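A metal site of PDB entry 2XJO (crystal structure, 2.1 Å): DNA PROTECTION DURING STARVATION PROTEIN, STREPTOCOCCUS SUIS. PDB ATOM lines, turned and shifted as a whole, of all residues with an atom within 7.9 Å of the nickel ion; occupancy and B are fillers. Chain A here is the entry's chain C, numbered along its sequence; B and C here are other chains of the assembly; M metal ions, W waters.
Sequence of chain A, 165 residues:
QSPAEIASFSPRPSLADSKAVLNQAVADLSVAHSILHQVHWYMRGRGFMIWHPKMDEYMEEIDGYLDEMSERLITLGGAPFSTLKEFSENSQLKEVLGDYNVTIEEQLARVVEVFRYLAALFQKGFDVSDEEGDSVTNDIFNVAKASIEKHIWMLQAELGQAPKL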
ATOM      1  N   ASP A  63       0.828  -5.217  10.717  1.00  0.00           N
ATOM      2  CA  ASP A  63      -0.536  -5.225  11.268  1.00  0.00           C
ATOM      3  C   ASP A  63      -0.605  -5.857  12.675  1.00  0.00           C
ATOM      4  O   ASP A  63      -1.429  -5.451  13.507  1.00  0.00           O
ATOM      5  CB  ASP A  63      -1.538  -5.913  10.313  1.00  0.00           C
ATOM      6  CG  ASP A  63      -1.993  -4.999   9.139  1.00  0.00           C
ATOM      7  OD1 ASP A  63      -2.218  -5.563   8.031  1.00  0.00           O
ATOM      8  OD2 ASP A  63      -2.131  -3.724   9.295  1.00  0.00           O
ATOM      9  N   LEU A  66       0.479  -3.085  15.039  1.00  0.00           N
ATOM     10  CA  LEU A  66      -0.633  -2.180  15.031  1.00  0.00           C
ATOM     11  C   LEU A  66      -1.721  -2.611  15.990  1.00  0.00           C
ATOM     12  O   LEU A  66      -2.137  -1.828  16.849  1.00  0.00           O
ATOM     13  CB  LEU A  66      -1.192  -2.034  13.609  1.00  0.00           C
ATOM     14  CG  LEU A  66      -2.275  -1.005  13.201  1.00  0.00           C
ATOM     15  CD1 LEU A  66      -2.390   0.195  14.154  1.00  0.00           C
ATOM     16  CD2 LEU A  66      -2.061  -0.511  11.730  1.00  0.00           C
ATOM     17  N   ASP A  67      -2.174  -3.865  15.871  1.00  0.00           N
ATOM     18  CA  ASP A  67      -3.327  -4.294  16.643  1.00  0.00           C
ATOM     19  C   ASP A  67      -2.978  -4.412  18.135  1.00  0.00           C
ATOM     20  O   ASP A  67      -3.721  -3.968  19.009  1.00  0.00           O
ATOM     21  CB  ASP A  67      -3.990  -5.566  16.091  1.00  0.00           C
ATOM     22  CG  ASP A  67      -5.412  -5.749  16.635  1.00  0.00           C
ATOM     23  OD1 ASP A  67      -5.663  -6.754  17.379  1.00  0.00           O
ATOM     24  OD2 ASP A  67      -6.278  -4.858  16.366  1.00  0.00           O
ATOM     25  N   GLU A  68      -1.808  -4.948  18.397  1.00  0.00           N
ATOM     26  CA  GLU A  68      -1.301  -5.087  19.713  1.00  0.00           C
ATOM     27  C   GLU A  68      -1.085  -3.736  20.434  1.00  0.00           C
ATOM     28  O   GLU A  68      -1.369  -3.591  21.623  1.00  0.00           O
ATOM     29  CB  GLU A  68       0.005  -5.804  19.551  1.00  0.00           C
ATOM     30  CG  GLU A  68       0.859  -5.872  20.742  1.00  0.00           C
ATOM     31  CD  GLU A  68       1.886  -6.966  20.572  1.00  0.00           C
ATOM     32  OE1 GLU A  68       2.666  -6.859  19.579  1.00  0.00           O
ATOM     33  OE2 GLU A  68       1.867  -7.906  21.414  1.00  0.00           O
ATOM     34  N   SER A  70      -2.454  -0.665  19.681  1.00  0.00           N
ATOM     35  CA  SER A  70      -3.677   0.100  19.920  1.00  0.00           C
ATOM     36  C   SER A  70      -4.438  -0.504  21.096  1.00  0.00           C
ATOM     37  O   SER A  70      -5.014   0.217  21.908  1.00  0.00           O
ATOM     38  CB  SER A  70      -4.571   0.160  18.679  1.00  0.00           C
ATOM     39  OG  SER A  70      -4.955  -1.159  18.284  1.00  0.00           O
ATOM     40  N   GLU A  71      -4.410  -1.816  21.205  1.00  0.00           N
ATOM     41  CA  GLU A  71      -5.129  -2.466  22.285  1.00  0.00           C
ATOM     42  C   GLU A  71      -4.440  -2.352  23.625  1.00  0.00           C
ATOM     43  O   GLU A  71      -5.109  -2.372  24.653  1.00  0.00           O
ATOM     44  CB  GLU A  71      -5.411  -3.912  21.932  1.00  0.00           C
ATOM     45  CG  GLU A  71      -6.552  -3.947  20.942  1.00  0.00           C
ATOM     46  CD  GLU A  71      -6.602  -5.196  20.120  1.00  0.00           C
ATOM     47  OE1 GLU A  71      -6.048  -6.250  20.576  1.00  0.00           O
ATOM     48  OE2 GLU A  71      -7.211  -5.078  19.018  1.00  0.00           O
ATOM     49  N   ILE A  74      -5.759   1.019  24.338  1.00  0.00           N
ATOM     50  CA  ILE A  74      -7.130   0.935  24.852  1.00  0.00           C
ATOM     51  C   ILE A  74      -7.076   0.429  26.313  1.00  0.00           C
ATOM     52  O   ILE A  74      -7.735   0.977  27.192  1.00  0.00           O
ATOM     53  CB  ILE A  74      -8.029   0.004  23.974  1.00  0.00           C
ATOM     54  CG1 ILE A  74      -8.123   0.534  22.553  1.00  0.00           C
ATOM     55  CG2 ILE A  74      -9.452  -0.084  24.595  1.00  0.00           C
ATOM     56  CD1 ILE A  74      -8.543  -0.529  21.519  1.00  0.00           C
ATOM     57  N   HIS B  37     -11.739  -1.241  11.911  1.00  0.00           N
ATOM     58  CA  HIS B  37     -10.783  -1.132  12.986  1.00  0.00           C
ATOM     59  C   HIS B  37     -11.334  -0.296  14.153  1.00  0.00           C
ATOM     60  O   HIS B  37     -11.289  -0.702  15.318  1.00  0.00           O
ATOM     61  CB  HIS B  37      -9.484  -0.525  12.457  1.00  0.00           C
ATOM     62  CG  HIS B  37      -8.345  -1.488  12.448  1.00  0.00           C
ATOM     63  ND1 HIS B  37      -8.113  -2.370  13.501  1.00  0.00           N
ATOM     64  CD2 HIS B  37      -7.374  -1.726  11.539  1.00  0.00           C
ATOM     65  CE1 HIS B  37      -7.040  -3.090  13.226  1.00  0.00           C
ATOM     66  NE2 HIS B  37      -6.578  -2.727  12.046  1.00  0.00           N
ATOM     67  N   HIS B  40     -13.967  -2.110  15.925  1.00  0.00           N
ATOM     68  CA  HIS B  40     -13.282  -3.147  16.645  1.00  0.00           C
ATOM     69  C   HIS B  40     -12.688  -2.612  17.962  1.00  0.00           C
ATOM     70  O   HIS B  40     -12.875  -3.206  19.020  1.00  0.00           O
ATOM     71  CB  HIS B  40     -12.212  -3.698  15.704  1.00  0.00           C
ATOM     72  CG  HIS B  40     -11.315  -4.729  16.278  1.00  0.00           C
ATOM     73  ND1 HIS B  40     -11.712  -6.043  16.467  1.00  0.00           N
ATOM     74  CD2 HIS B  40      -9.994  -4.700  16.565  1.00  0.00           C
ATOM     75  CE1 HIS B  40     -10.687  -6.750  16.907  1.00  0.00           C
ATOM     76  NE2 HIS B  40      -9.640  -5.962  16.967  1.00  0.00           N
ATOM     77  N   TRP B  41     -11.986  -1.484  17.898  1.00  0.00           N
ATOM     78  CA  TRP B  41     -11.348  -0.913  19.082  1.00  0.00           C
ATOM     79  C   TRP B  41     -12.302  -0.280  20.131  1.00  0.00           C
ATOM     80  O   TRP B  41     -12.127  -0.475  21.343  1.00  0.00           O
ATOM     81  CB  TRP B  41     -10.319   0.112  18.633  1.00  0.00           C
ATOM     82  CG  TRP B  41      -9.151  -0.490  17.936  1.00  0.00           C
ATOM     83  CD1 TRP B  41      -8.631  -1.750  18.117  1.00  0.00           C
ATOM     84  CD2 TRP B  41      -8.329   0.155  16.957  1.00  0.00           C
ATOM     85  NE1 TRP B  41      -7.523  -1.932  17.325  1.00  0.00           N
ATOM     86  CE2 TRP B  41      -7.334  -0.787  16.582  1.00  0.00           C
ATOM     87  CE3 TRP B  41      -8.330   1.424  16.365  1.00  0.00           C
ATOM     88  CZ2 TRP B  41      -6.339  -0.494  15.627  1.00  0.00           C
ATOM     89  CZ3 TRP B  41      -7.318   1.726  15.419  1.00  0.00           C
ATOM     90  CH2 TRP B  41      -6.346   0.778  15.062  1.00  0.00           C
ATOM     91  N   HIS B  52     -16.488  -8.152  18.591  1.00  0.00           N
ATOM     92  CA  HIS B  52     -15.124  -7.682  18.504  1.00  0.00           C
ATOM     93  C   HIS B  52     -14.254  -8.543  17.543  1.00  0.00           C
ATOM     94  O   HIS B  52     -13.653  -7.965  16.621  1.00  0.00           O
ATOM     95  CB  HIS B  52     -14.499  -7.521  19.898  1.00  0.00           C
ATOM     96  CG  HIS B  52     -13.012  -7.326  19.903  1.00  0.00           C
ATOM     97  ND1 HIS B  52     -12.427  -6.076  19.766  1.00  0.00           N
ATOM     98  CD2 HIS B  52     -11.996  -8.201  20.077  1.00  0.00           C
ATOM     99  CE1 HIS B  52     -11.113  -6.209  19.831  1.00  0.00           C
ATOM    100  NE2 HIS B  52     -10.822  -7.476  20.039  1.00  0.00           N
ATOM    101  N   PRO B  53     -14.173  -9.883  17.753  1.00  0.00           N
ATOM    102  CA  PRO B  53     -13.413 -10.710  16.766  1.00  0.00           C
ATOM    103  C   PRO B  53     -14.098 -10.819  15.405  1.00  0.00           C
ATOM    104  O   PRO B  53     -13.420 -11.030  14.412  1.00  0.00           O
ATOM    105  CB  PRO B  53     -13.313 -12.095  17.420  1.00  0.00           C
ATOM    106  CG  PRO B  53     -14.481 -12.110  18.433  1.00  0.00           C
ATOM    107  CD  PRO B  53     -14.565 -10.684  18.939  1.00  0.00           C
ATOM    108  N   MET B  55     -15.314  -8.281  13.792  1.00  0.00           N
ATOM    109  CA  MET B  55     -14.731  -7.197  12.991  1.00  0.00           C
ATOM    110  C   MET B  55     -13.409  -7.651  12.345  1.00  0.00           C
ATOM    111  O   MET B  55     -13.054  -7.195  11.263  1.00  0.00           O
ATOM    112  CB  MET B  55     -14.478  -5.911  13.806  1.00  0.00           C
ATOM    113  CG  MET B  55     -15.745  -5.155  14.328  1.00  0.00           C
ATOM    114  SD  MET B  55     -16.998  -4.946  13.040  1.00  0.00           S
ATOM    115  CE  MET B  55     -18.287  -6.042  13.590  1.00  0.00           C
ATOM    116  N   ASP B  56     -12.659  -8.510  13.037  1.00  0.00           N
ATOM    117  CA  ASP B  56     -11.456  -9.108  12.427  1.00  0.00           C
ATOM    118  C   ASP B  56     -11.776  -9.897  11.150  1.00  0.00           C
ATOM    119  O   ASP B  56     -11.061  -9.776  10.172  1.00  0.00           O
ATOM    120  CB  ASP B  56     -10.741 -10.066  13.383  1.00  0.00           C
ATOM    121  CG  ASP B  56      -9.735  -9.386  14.216  1.00  0.00           C
ATOM    122  OD1 ASP B  56      -9.748  -9.621  15.459  1.00  0.00           O
ATOM    123  OD2 ASP B  56      -8.916  -8.650  13.633  1.00  0.00           O
ATOM    124  N   MET B  59     -12.577  -7.442   8.339  1.00  0.00           N
ATOM    125  CA  MET B  59     -11.370  -6.759   7.884  1.00  0.00           C
ATOM    126  C   MET B  59     -10.506  -7.617   6.951  1.00  0.00           C
ATOM    127  O   MET B  59      -9.977  -7.109   5.949  1.00  0.00           O
ATOM    128  CB  MET B  59     -10.555  -6.257   9.076  1.00  0.00           C
ATOM    129  CG  MET B  59     -11.166  -4.987   9.666  1.00  0.00           C
ATOM    130  SD  MET B  59     -10.181  -4.178  10.923  1.00  0.00           S
ATOM    131  CE  MET B  59     -10.584  -5.140  12.378  1.00  0.00           C
ATOM    132  N   LYS C 150      -5.185  -7.506  29.276  1.00  0.00           N
ATOM    133  CA  LYS C 150      -5.914  -7.576  28.018  1.00  0.00           C
ATOM    134  C   LYS C 150      -7.320  -8.146  28.304  1.00  0.00           C
ATOM    135  O   LYS C 150      -8.309  -7.597  27.845  1.00  0.00           O
ATOM    136  CB  LYS C 150      -5.134  -8.435  26.995  1.00  0.00           C
ATOM    137  CG  LYS C 150      -5.628  -8.425  25.550  1.00  0.00           C
ATOM    138  CD  LYS C 150      -4.561  -8.863  24.481  1.00  0.00           C
ATOM    139  CE  LYS C 150      -3.830  -7.662  23.769  1.00  0.00           C
ATOM    140  NZ  LYS C 150      -4.242  -7.300  22.309  1.00  0.00           N
ATOM    141  N   TRP C 153      -9.572  -5.481  30.008  1.00  0.00           N
ATOM    142  CA  TRP C 153     -10.174  -4.620  28.976  1.00  0.00           C
ATOM    143  C   TRP C 153     -11.412  -5.260  28.324  1.00  0.00           C
ATOM    144  O   TRP C 153     -12.497  -4.678  28.292  1.00  0.00           O
ATOM    145  CB  TRP C 153      -9.140  -4.195  27.927  1.00  0.00           C
ATOM    146  CG  TRP C 153      -9.741  -3.901  26.567  1.00  0.00           C
ATOM    147  CD1 TRP C 153     -10.767  -3.039  26.291  1.00  0.00           C
ATOM    148  CD2 TRP C 153      -9.364  -4.492  25.316  1.00  0.00           C
ATOM    149  NE1 TRP C 153     -11.052  -3.051  24.935  1.00  0.00           N
ATOM    150  CE2 TRP C 153     -10.209  -3.936  24.327  1.00  0.00           C
ATOM    151  CE3 TRP C 153      -8.409  -5.428  24.940  1.00  0.00           C
ATOM    152  CZ2 TRP C 153     -10.101  -4.295  22.966  1.00  0.00           C
ATOM    153  CZ3 TRP C 153      -8.304  -5.786  23.593  1.00  0.00           C
ATOM    154  CH2 TRP C 153      -9.156  -5.213  22.630  1.00  0.00           C
ATOM    155  N   MET C 154     -11.239  -6.469  27.812  1.00  0.00           N
ATOM    156  CA  MET C 154     -12.308  -7.166  27.099  1.00  0.00           C
ATOM    157  C   MET C 154     -13.540  -7.432  27.952  1.00  0.00           C
ATOM    158  O   MET C 154     -14.662  -7.181  27.493  1.00  0.00           O
ATOM    159  CB  MET C 154     -11.795  -8.478  26.501  1.00  0.00           C
ATOM    160  CG  MET C 154     -10.958  -8.240  25.272  1.00  0.00           C
ATOM    161  SD  MET C 154     -10.766  -9.754  24.348  1.00  0.00           S
ATOM    162  CE  MET C 154      -9.634  -9.175  23.062  1.00  0.00           C
HETATM  163 NI    NI M   1      -7.845  -6.656  17.642  1.00  0.00          NI
HETATM  164  O   HOH W   1      -7.751  -8.426  16.473  1.00  0.00           O
HETATM  165  O   HOH W   2      -8.252  -7.915  19.529  1.00  0.00           O
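ND1 of His 40 of chain B lies within hydrogen-bond range of O of His 52 of chain B. The side-chain carboxylate (OE1) of Glu 71 lies within salt-bridge range of the side-chain amino group (NZ) of Lys 150 of chain C, 2.7 Å away. The side-chain carboxylate (OD2) of Asp 67 sits at hydrogen-bond distance from the indole nitrogen (NE1) of Trp 41 of chain B. O of Asp 67 sits at hydrogen-bond distance from OG of Ser 70 (3.2 Å).
Residues that only touch the nickel ion: His 52 of chain B (3.9 Å). Four residues have an atom within 4 Å of the nickel ion: Asp 67, Glu 71, His 40 of chain B and His 52 of chain B. Along chain A the residues within 4 Å of the nickel ion span positions 67 to 71. The nearest printed residue that does not touch the nickel ion is Asp 56 of chain B (4.1 Å).
The nickel ion is bound by NE2 of His 40 of chain B (2.0 Å), water W1 (2.1 Å), OE2 of Glu 71 (2.2 Å), OD1 of Asp 67 (2.2 Å) and water W2 (2.3 Å). Slightly farther from the nickel ion lies the side-chain carboxylate (OD2) of Asp 67 (2.7 Å).
Water W2 lies within hydrogen-bond range of NE2 of His 52 of chain B (2.7 Å) and OE1 of Glu 71 (3.0 Å).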
